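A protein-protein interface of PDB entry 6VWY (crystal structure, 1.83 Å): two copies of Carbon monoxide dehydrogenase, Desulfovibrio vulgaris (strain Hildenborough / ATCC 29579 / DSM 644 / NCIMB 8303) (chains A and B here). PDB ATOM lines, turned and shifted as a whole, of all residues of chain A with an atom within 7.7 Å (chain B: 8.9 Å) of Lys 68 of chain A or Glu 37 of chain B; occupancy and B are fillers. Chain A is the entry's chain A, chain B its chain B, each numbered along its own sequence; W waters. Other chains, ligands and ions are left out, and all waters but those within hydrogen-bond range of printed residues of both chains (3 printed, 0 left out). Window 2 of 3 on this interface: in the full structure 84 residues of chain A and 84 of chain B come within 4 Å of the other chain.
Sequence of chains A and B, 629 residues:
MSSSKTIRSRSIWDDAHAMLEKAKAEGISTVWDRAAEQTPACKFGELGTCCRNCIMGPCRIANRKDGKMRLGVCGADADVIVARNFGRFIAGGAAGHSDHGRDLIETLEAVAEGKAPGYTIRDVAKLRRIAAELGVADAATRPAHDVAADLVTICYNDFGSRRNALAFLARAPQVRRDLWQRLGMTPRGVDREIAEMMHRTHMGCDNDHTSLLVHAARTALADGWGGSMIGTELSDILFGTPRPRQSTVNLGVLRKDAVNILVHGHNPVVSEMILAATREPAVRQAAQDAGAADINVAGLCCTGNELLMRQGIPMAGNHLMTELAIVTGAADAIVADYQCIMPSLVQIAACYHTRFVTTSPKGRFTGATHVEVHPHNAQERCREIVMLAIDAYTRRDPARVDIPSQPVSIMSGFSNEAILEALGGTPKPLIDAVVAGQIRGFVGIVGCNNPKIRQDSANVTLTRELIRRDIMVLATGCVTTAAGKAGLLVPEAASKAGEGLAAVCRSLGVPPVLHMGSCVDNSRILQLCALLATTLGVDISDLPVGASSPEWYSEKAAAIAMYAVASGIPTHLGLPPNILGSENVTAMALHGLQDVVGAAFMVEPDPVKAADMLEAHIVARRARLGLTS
Water W3 bridges OE1 of Gln 38 of chain B (2.5 Å) and NH2 of Arg 60 of chain A (3.0 Å). Water W1 lies within hydrogen-bond range of O of Leu 71 of chain A (2.7 Å), OE1 of Glu 37 of chain B (2.7 Å) and NE2 of Gln 38 of chain B (3.4 Å). Water W2 lies within hydrogen-bond range of the side-chain carboxylate (OE1) of Glu 37 of chain B, the backbone NH (N) of Arg 70 of chain A, the backbone NH (N) of Leu 71 of chain A and the backbone carbonyl oxygen (O) of Gly 67 of chain A.
No position is printed for both chains. Of the 11 pairs that touch across the chains among the printed residues, none has its exchanged pair printed and touching as well.
Hydrophobic or aromatic side chains of chain A that line the printed part of chain B: Met 69 and Val 73. Of the 14 printed residues of chain B, 6 touch a printed residue of chain A. Hydrophobic or aromatic side chains of chain B that line the printed part of chain A: Val 31 and Ala 35. Among the printed residues, 11 pairs touch across the chains. Among the printed residues, no Asp or Glu carboxylate lies within 4 Å of a Lys or Arg side-chain nitrogen of the other chain.
Lys 68 of chain A touches Glu 37 of chain B (CD to OE2, 3.3 Å). Gln 38 of chain B touches Met 69 of chain A (OE1 to CE, 3.5 Å). Val 31 of chain B touches Val 73 of chain A. Val 73 of chain A touches Ala 35 of chain B. CG2 of Val 73 of chain A touches CG of Gln 38 of chain B, 3.9 Å away.
N of Met 69 of chain A is in hydrogen-bond range of OE1 of Glu 37 of chain B, at 3.0 Å. O of Gly 72 of chain A is in hydrogen-bond range of NE of Arg 34 of chain B (3.4 Å). The backbone NH (N) of Arg 60 of chain A is in hydrogen-bond range of the side-chain amide oxygen (OE1) of Gln 38 of chain B (3.0 Å). NE of Arg 34 of chain B is in hydrogen-bond range of O of Val 73 of chain A, 2.8 Å away. The guanidinium group (NH2) of Arg 60 of chain A is in hydrogen-bond range of the backbone carbonyl oxygen (O) of Pro 40 of chain B (3.5 Å). The side-chain amide nitrogen of Gln 38 of chain B sits at hydrogen-bond distance from the backbone carbonyl oxygen of Leu 71 of chain A (3.2 Å).
No residue of chain B comes within 4 Å of Asp 66 of chain A. No residue of chain B comes within 4 Å of Gly 67 of chain A. Of chain B, only Glu 37 (3.3 Å) comes within 4 Å of Lys 68 of chain A. Of chain B, only Glu 37 and Gln 38 come within 4 Å of Met 69 of chain A. Printed residues of chain B within 4 Å of Leu 71 of chain A: Gln 38. Of the printed residues of chain B, Val 73 of chain A touches Val 31 (3.6 Å), Arg 34 (2.8 Å), Ala 35 (3.7 Å) and Gln 38 (3.9 Å). Ser 29 of chain B touches none of the printed residues of chain A. Printed residues of chain A within 4 Å of Arg 34 of chain B: Gly 72 and Val 73. Of the printed residues of chain A, Ala 35 of chain B touches Val 73 (3.7 Å). No residue of chain A comes within 4 Å of Ala 36 of chain B. Of the printed residues of chain A, Gln 38 of chain B touches Arg 60, Met 69, Leu 71 and Val 73. The nearest residue of chain B that does not touch Lys 68 of chain A is Gln 38 of chain B (6.4 Å).
OG1 of Thr 39 of chain B is in hydrogen-bond range of O of Ala 35 of chain B (2.7 Å). N of Ala 62 of chain A is in hydrogen-bond range of O of Met 69 of chain A, 3.0 Å away. The backbone NH of Lys 68 of chain A lies within hydrogen-bond range of the side-chain carboxylate of Asp 66 of chain A (3.0 Å). The backbone carbonyl oxygen of Thr 30 of chain B lies close to the guanidinium group of Arg 34 of chain B, at 3.5 Å.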
ATOM      1  N   ARG A  60      10.743  15.500  11.331  1.00  0.00           N
ATOM      2  CA  ARG A  60      11.236  14.540  12.304  1.00  0.00           C
ATOM      3  C   ARG A  60      10.850  13.141  11.846  1.00  0.00           C
ATOM      4  O   ARG A  60       9.791  12.943  11.245  1.00  0.00           O
ATOM      5  CB  ARG A  60      10.714  14.843  13.720  1.00  0.00           C
ATOM      6  CG  ARG A  60       9.209  14.887  13.853  1.00  0.00           C
ATOM      7  CD  ARG A  60       8.765  15.480  15.206  1.00  0.00           C
ATOM      8  NE  ARG A  60       7.379  15.097  15.479  1.00  0.00           N
ATOM      9  CZ  ARG A  60       6.311  15.738  15.018  1.00  0.00           C
ATOM     10  NH1 ARG A  60       5.099  15.291  15.311  1.00  0.00           N
ATOM     11  NH2 ARG A  60       6.448  16.821  14.267  1.00  0.00           N
ATOM     12  N   ILE A  61      11.729  12.177  12.129  1.00  0.00           N
ATOM     13  CA  ILE A  61      11.582  10.800  11.668  1.00  0.00           C
ATOM     14  C   ILE A  61      11.193   9.951  12.865  1.00  0.00           C
ATOM     15  O   ILE A  61      11.918   9.907  13.863  1.00  0.00           O
ATOM     16  CB  ILE A  61      12.878  10.273  11.032  1.00  0.00           C
ATOM     17  CG1 ILE A  61      13.384  11.239   9.963  1.00  0.00           C
ATOM     18  CG2 ILE A  61      12.663   8.862  10.478  1.00  0.00           C
ATOM     19  CD1 ILE A  61      12.392  11.467   8.820  1.00  0.00           C
ATOM     20  N   ALA A  62      10.054   9.286  12.770  1.00  0.00           N
ATOM     21  CA  ALA A  62       9.632   8.313  13.760  1.00  0.00           C
ATOM     22  C   ALA A  62       9.810   6.908  13.198  1.00  0.00           C
ATOM     23  O   ALA A  62      10.023   6.707  12.000  1.00  0.00           O
ATOM     24  CB  ALA A  62       8.178   8.555  14.166  1.00  0.00           C
ATOM     25  N   ASN A  63       9.722   5.925  14.085  1.00  0.00           N
ATOM     26  CA  ASN A  63       9.797   4.515  13.717  1.00  0.00           C
ATOM     27  C   ASN A  63       8.397   3.935  13.892  1.00  0.00           C
ATOM     28  O   ASN A  63       8.071   3.350  14.921  1.00  0.00           O
ATOM     29  CB  ASN A  63      10.832   3.795  14.579  1.00  0.00           C
ATOM     30  CG  ASN A  63      11.147   2.407  14.074  1.00  0.00           C
ATOM     31  OD1 ASN A  63      11.415   2.209  12.888  1.00  0.00           O
ATOM     32  ND2 ASN A  63      11.111   1.429  14.974  1.00  0.00           N
ATOM     33  N   ARG A  64       7.554   4.123  12.880  1.00  0.00           N
ATOM     34  CA  ARG A  64       6.143   3.777  12.979  1.00  0.00           C
ATOM     35  C   ARG A  64       5.803   2.579  12.103  1.00  0.00           C
ATOM     36  O   ARG A  64       6.256   2.478  10.954  1.00  0.00           O
ATOM     37  CB  ARG A  64       5.256   4.960  12.600  1.00  0.00           C
ATOM     38  CG  ARG A  64       5.306   6.111  13.592  1.00  0.00           C
ATOM     39  CD  ARG A  64       4.282   7.172  13.230  1.00  0.00           C
ATOM     40  NE  ARG A  64       2.925   6.740  13.554  1.00  0.00           N
ATOM     41  CZ  ARG A  64       1.823   7.388  13.191  1.00  0.00           C
ATOM     42  NH1 ARG A  64       0.632   6.914  13.532  1.00  0.00           N
ATOM     43  NH2 ARG A  64       1.907   8.504  12.482  1.00  0.00           N
ATOM     44  N   LYS A  65       4.981   1.680  12.651  1.00  0.00           N
ATOM     45  CA  LYS A  65       4.615   0.479  11.913  1.00  0.00           C
ATOM     46  C   LYS A  65       3.822   0.816  10.656  1.00  0.00           C
ATOM     47  O   LYS A  65       3.931   0.106   9.651  1.00  0.00           O
ATOM     48  CB  LYS A  65       3.832  -0.483  12.818  1.00  0.00           C
ATOM     49  N   ASP A  66       3.044   1.903  10.675  1.00  0.00           N
ATOM     50  CA  ASP A  66       2.301   2.284   9.480  1.00  0.00           C
ATOM     51  C   ASP A  66       3.149   3.039   8.462  1.00  0.00           C
ATOM     52  O   ASP A  66       2.613   3.469   7.439  1.00  0.00           O
ATOM     53  CB  ASP A  66       1.055   3.102   9.853  1.00  0.00           C
ATOM     54  CG  ASP A  66       1.381   4.479  10.411  1.00  0.00           C
ATOM     55  OD1 ASP A  66       2.573   4.809  10.602  1.00  0.00           O
ATOM     56  OD2 ASP A  66       0.418   5.242  10.658  1.00  0.00           O
ATOM     57  N   GLY A  67       4.449   3.208   8.706  1.00  0.00           N
ATOM     58  CA  GLY A  67       5.314   3.848   7.737  1.00  0.00           C
ATOM     59  C   GLY A  67       5.195   5.356   7.646  1.00  0.00           C
ATOM     60  O   GLY A  67       5.880   5.961   6.811  1.00  0.00           O
ATOM     61  N   LYS A  68       4.361   5.981   8.473  1.00  0.00           N
ATOM     62  CA  LYS A  68       4.230   7.432   8.461  1.00  0.00           C
ATOM     63  C   LYS A  68       5.421   8.078   9.156  1.00  0.00           C
ATOM     64  O   LYS A  68       6.020   7.506  10.074  1.00  0.00           O
ATOM     65  CB  LYS A  68       2.935   7.869   9.146  1.00  0.00           C
ATOM     66  CG  LYS A  68       1.659   7.442   8.438  1.00  0.00           C
ATOM     67  CD  LYS A  68       1.280   8.410   7.338  1.00  0.00           C
ATOM     68  CE  LYS A  68      -0.180   8.241   6.939  1.00  0.00           C
ATOM     69  NZ  LYS A  68      -1.104   8.477   8.090  1.00  0.00           N
ATOM     70  N   MET A  69       5.762   9.282   8.694  1.00  0.00           N
ATOM     71  CA  MET A  69       6.918  10.036   9.172  1.00  0.00           C
ATOM     72  C   MET A  69       8.194   9.210   9.097  1.00  0.00           C
ATOM     73  O   MET A  69       9.092   9.347   9.929  1.00  0.00           O
ATOM     74  CB  MET A  69       6.676  10.570  10.585  1.00  0.00           C
ATOM     75  CG  MET A  69       5.394  11.385  10.652  1.00  0.00           C
ATOM     76  SD  MET A  69       5.112  12.180  12.227  1.00  0.00           S
ATOM     77  CE  MET A  69       6.170  13.609  12.049  1.00  0.00           C
ATOM     78  N   ARG A  70       8.284   8.352   8.080  1.00  0.00           N
ATOM     79  CA  ARG A  70       9.528   7.638   7.824  1.00  0.00           C
ATOM     80  C   ARG A  70      10.533   8.512   7.083  1.00  0.00           C
ATOM     81  O   ARG A  70      11.746   8.296   7.208  1.00  0.00           O
ATOM     82  CB  ARG A  70       9.248   6.363   7.018  1.00  0.00           C
ATOM     83  CG  ARG A  70      10.478   5.478   6.859  1.00  0.00           C
ATOM     84  CD  ARG A  70      10.178   4.162   6.177  1.00  0.00           C
ATOM     85  NE  ARG A  70       9.731   4.317   4.795  1.00  0.00           N
ATOM     86  CZ  ARG A  70      10.545   4.455   3.751  1.00  0.00           C
ATOM     87  NH1 ARG A  70      11.864   4.478   3.920  1.00  0.00           N
ATOM     88  NH2 ARG A  70      10.038   4.578   2.535  1.00  0.00           N
ATOM     89  N   LEU A  71      10.055   9.496   6.316  1.00  0.00           N
ATOM     90  CA  LEU A  71      10.906  10.332   5.482  1.00  0.00           C
ATOM     91  C   LEU A  71      10.622  11.804   5.764  1.00  0.00           C
ATOM     92  O   LEU A  71       9.518  12.172   6.164  1.00  0.00           O
ATOM     93  CB  LEU A  71      10.677  10.042   3.988  1.00  0.00           C
ATOM     94  CG  LEU A  71      10.786   8.582   3.525  1.00  0.00           C
ATOM     95  CD1 LEU A  71      10.341   8.418   2.056  1.00  0.00           C
ATOM     96  CD2 LEU A  71      12.204   8.064   3.733  1.00  0.00           C
ATOM     97  N   GLY A  72      11.627  12.644   5.558  1.00  0.00           N
ATOM     98  CA  GLY A  72      11.401  14.076   5.588  1.00  0.00           C
ATOM     99  C   GLY A  72      10.602  14.508   4.369  1.00  0.00           C
ATOM    100  O   GLY A  72      10.293  13.724   3.469  1.00  0.00           O
ATOM    101  N   VAL A  73      10.264  15.796   4.324  1.00  0.00           N
ATOM    102  CA  VAL A  73       9.408  16.250   3.220  1.00  0.00           C
ATOM    103  C   VAL A  73      10.111  16.051   1.877  1.00  0.00           C
ATOM    104  O   VAL A  73       9.476  15.688   0.877  1.00  0.00           O
ATOM    105  CB  VAL A  73       8.974  17.713   3.435  1.00  0.00           C
ATOM    106  CG1 VAL A  73       8.173  18.214   2.226  1.00  0.00           C
ATOM    107  CG2 VAL A  73       8.138  17.836   4.715  1.00  0.00           C
ATOM    108  N   ARG B  10      -3.127  22.075  -4.423  1.00  0.00           N
ATOM    109  CA  ARG B  10      -1.680  21.915  -4.313  1.00  0.00           C
ATOM    110  C   ARG B  10      -0.899  22.623  -5.411  1.00  0.00           C
ATOM    111  O   ARG B  10       0.303  22.880  -5.240  1.00  0.00           O
ATOM    112  CB  ARG B  10      -1.336  20.424  -4.308  1.00  0.00           C
ATOM    113  CG  ARG B  10      -1.786  19.773  -3.011  1.00  0.00           C
ATOM    114  CD  ARG B  10      -1.639  18.280  -3.013  1.00  0.00           C
ATOM    115  NE  ARG B  10      -1.818  17.754  -1.665  1.00  0.00           N
ATOM    116  CZ  ARG B  10      -1.729  16.466  -1.354  1.00  0.00           C
ATOM    117  NH1 ARG B  10      -1.466  15.568  -2.302  1.00  0.00           N
ATOM    118  NH2 ARG B  10      -1.900  16.076  -0.098  1.00  0.00           N
ATOM    119  N   SER B  29       3.472   8.257  -3.370  1.00  0.00           N
ATOM    120  CA  SER B  29       3.429   9.392  -2.456  1.00  0.00           C
ATOM    121  C   SER B  29       4.376  10.487  -2.937  1.00  0.00           C
ATOM    122  O   SER B  29       5.474  10.209  -3.424  1.00  0.00           O
ATOM    123  CB  SER B  29       3.790   8.960  -1.028  1.00  0.00           C
ATOM    124  OG  SER B  29       5.177   9.093  -0.788  1.00  0.00           O
ATOM    125  N   THR B  30       3.946  11.732  -2.798  1.00  0.00           N
ATOM    126  CA  THR B  30       4.705  12.864  -3.314  1.00  0.00           C
ATOM    127  C   THR B  30       5.154  13.749  -2.163  1.00  0.00           C
ATOM    128  O   THR B  30       4.838  13.501  -0.997  1.00  0.00           O
ATOM    129  CB  THR B  30       3.877  13.682  -4.307  1.00  0.00           C
ATOM    130  OG1 THR B  30       2.848  14.376  -3.593  1.00  0.00           O
ATOM    131  CG2 THR B  30       3.233  12.770  -5.341  1.00  0.00           C
ATOM    132  N   VAL B  31       5.871  14.815  -2.528  1.00  0.00           N
ATOM    133  CA  VAL B  31       6.323  15.806  -1.555  1.00  0.00           C
ATOM    134  C   VAL B  31       5.146  16.376  -0.770  1.00  0.00           C
ATOM    135  O   VAL B  31       5.259  16.646   0.434  1.00  0.00           O
ATOM    136  CB  VAL B  31       7.121  16.912  -2.271  1.00  0.00           C
ATOM    137  CG1 VAL B  31       6.286  17.544  -3.410  1.00  0.00           C
ATOM    138  CG2 VAL B  31       7.583  17.965  -1.285  1.00  0.00           C
ATOM    139  N   TRP B  32       3.999  16.566  -1.431  1.00  0.00           N
ATOM    140  CA  TRP B  32       2.829  17.111  -0.740  1.00  0.00           C
ATOM    141  C   TRP B  32       2.292  16.132   0.287  1.00  0.00           C
ATOM    142  O   TRP B  32       1.804  16.540   1.348  1.00  0.00           O
ATOM    143  CB  TRP B  32       1.715  17.450  -1.728  1.00  0.00           C
ATOM    144  CG  TRP B  32       1.939  18.661  -2.572  1.00  0.00           C
ATOM    145  CD1 TRP B  32       1.699  19.963  -2.224  1.00  0.00           C
ATOM    146  CD2 TRP B  32       2.433  18.687  -3.914  1.00  0.00           C
ATOM    147  NE1 TRP B  32       2.018  20.799  -3.275  1.00  0.00           N
ATOM    148  CE2 TRP B  32       2.465  20.041  -4.324  1.00  0.00           C
ATOM    149  CE3 TRP B  32       2.851  17.697  -4.813  1.00  0.00           C
ATOM    150  CZ2 TRP B  32       2.889  20.428  -5.595  1.00  0.00           C
ATOM    151  CZ3 TRP B  32       3.279  18.087  -6.077  1.00  0.00           C
ATOM    152  CH2 TRP B  32       3.297  19.438  -6.455  1.00  0.00           C
ATOM    153  N   ASP B  33       2.329  14.838  -0.029  1.00  0.00           N
ATOM    154  CA  ASP B  33       1.907  13.841   0.950  1.00  0.00           C
ATOM    155  C   ASP B  33       2.832  13.843   2.158  1.00  0.00           C
ATOM    156  O   ASP B  33       2.371  13.795   3.306  1.00  0.00           O
ATOM    157  CB  ASP B  33       1.861  12.465   0.302  1.00  0.00           C
ATOM    158  CG  ASP B  33       0.921  12.426  -0.887  1.00  0.00           C
ATOM    159  OD1 ASP B  33      -0.227  12.880  -0.733  1.00  0.00           O
ATOM    160  OD2 ASP B  33       1.335  11.964  -1.969  1.00  0.00           O
ATOM    161  N   ARG B  34       4.142  13.911   1.921  1.00  0.00           N
ATOM    162  CA  ARG B  34       5.078  13.896   3.037  1.00  0.00           C
ATOM    163  C   ARG B  34       4.988  15.182   3.840  1.00  0.00           C
ATOM    164  O   ARG B  34       5.114  15.152   5.066  1.00  0.00           O
ATOM    165  CB  ARG B  34       6.499  13.663   2.523  1.00  0.00           C
ATOM    166  CG  ARG B  34       6.669  12.266   1.878  1.00  0.00           C
ATOM    167  CD  ARG B  34       8.120  11.961   1.489  1.00  0.00           C
ATOM    168  NE  ARG B  34       8.673  12.993   0.618  1.00  0.00           N
ATOM    169  CZ  ARG B  34       8.578  13.000  -0.710  1.00  0.00           C
ATOM    170  NH1 ARG B  34       7.943  12.016  -1.352  1.00  0.00           N
ATOM    171  NH2 ARG B  34       9.120  13.994  -1.408  1.00  0.00           N
ATOM    172  N   ALA B  35       4.741  16.314   3.173  1.00  0.00           N
ATOM    173  CA  ALA B  35       4.507  17.561   3.898  1.00  0.00           C
ATOM    174  C   ALA B  35       3.293  17.449   4.818  1.00  0.00           C
ATOM    175  O   ALA B  35       3.300  17.971   5.938  1.00  0.00           O
ATOM    176  CB  ALA B  35       4.339  18.717   2.904  1.00  0.00           C
ATOM    177  N   ALA B  36       2.243  16.762   4.369  1.00  0.00           N
ATOM    178  CA  ALA B  36       1.076  16.554   5.221  1.00  0.00           C
ATOM    179  C   ALA B  36       1.412  15.674   6.424  1.00  0.00           C
ATOM    180  O   ALA B  36       0.930  15.924   7.536  1.00  0.00           O
ATOM    181  CB  ALA B  36      -0.063  15.943   4.402  1.00  0.00           C
ATOM    182  N   GLU B  37       2.244  14.645   6.228  1.00  0.00           N
ATOM    183  CA  GLU B  37       2.652  13.806   7.352  1.00  0.00           C
ATOM    184  C   GLU B  37       3.450  14.599   8.385  1.00  0.00           C
ATOM    185  O   GLU B  37       3.374  14.309   9.585  1.00  0.00           O
ATOM    186  CB  GLU B  37       3.486  12.621   6.864  1.00  0.00           C
ATOM    187  CG  GLU B  37       2.750  11.609   5.987  1.00  0.00           C
ATOM    188  CD  GLU B  37       3.630  10.421   5.619  1.00  0.00           C
ATOM    189  OE1 GLU B  37       4.801  10.384   6.056  1.00  0.00           O
ATOM    190  OE2 GLU B  37       3.156   9.526   4.887  1.00  0.00           O
ATOM    191  N   GLN B  38       4.231  15.584   7.942  1.00  0.00           N
ATOM    192  CA  GLN B  38       5.084  16.359   8.832  1.00  0.00           C
ATOM    193  C   GLN B  38       4.371  17.594   9.396  1.00  0.00           C
ATOM    194  O   GLN B  38       5.034  18.499   9.928  1.00  0.00           O
ATOM    195  CB  GLN B  38       6.378  16.758   8.105  1.00  0.00           C
ATOM    196  CG  GLN B  38       7.250  15.554   7.688  1.00  0.00           C
ATOM    197  CD  GLN B  38       7.991  14.941   8.874  1.00  0.00           C
ATOM    198  OE1 GLN B  38       8.136  15.571   9.927  1.00  0.00           O
ATOM    199  NE2 GLN B  38       8.466  13.714   8.704  1.00  0.00           N
ATOM    200  N   THR B  39       3.039  17.630   9.309  1.00  0.00           N
ATOM    201  CA  THR B  39       2.205  18.718   9.798  1.00  0.00           C
ATOM    202  C   THR B  39       1.270  18.198  10.882  1.00  0.00           C
ATOM    203  O   THR B  39       0.581  17.193  10.663  1.00  0.00           O
ATOM    204  CB  THR B  39       1.371  19.331   8.649  1.00  0.00           C
ATOM    205  OG1 THR B  39       2.247  19.757   7.602  1.00  0.00           O
ATOM    206  CG2 THR B  39       0.580  20.527   9.140  1.00  0.00           C
ATOM    207  N   PRO B  40       1.201  18.849  12.053  1.00  0.00           N
ATOM    208  CA  PRO B  40       1.961  20.053  12.400  1.00  0.00           C
ATOM    209  C   PRO B  40       3.398  19.741  12.798  1.00  0.00           C
ATOM    210  O   PRO B  40       3.684  18.684  13.361  1.00  0.00           O
ATOM    211  CB  PRO B  40       1.181  20.626  13.587  1.00  0.00           C
ATOM    212  CG  PRO B  40       0.621  19.421  14.264  1.00  0.00           C
ATOM    213  CD  PRO B  40       0.314  18.424  13.153  1.00  0.00           C
ATOM    214  N   ALA B  41       4.293  20.673  12.509  1.00  0.00           N
ATOM    215  CA  ALA B  41       5.705  20.507  12.785  1.00  0.00           C
ATOM    216  C   ALA B  41       6.029  20.995  14.196  1.00  0.00           C
ATOM    217  O   ALA B  41       5.242  21.693  14.839  1.00  0.00           O
ATOM    218  CB  ALA B  41       6.542  21.260  11.749  1.00  0.00           C
HETATM  219  O   HOH W   1       6.819  12.233   6.190  1.00  0.00           O
HETATM  220  O   HOH W   2       7.101   8.786   5.342  1.00  0.00           O
HETATM  221  O   HOH W   3       7.140  17.352  11.397  1.00  0.00           O
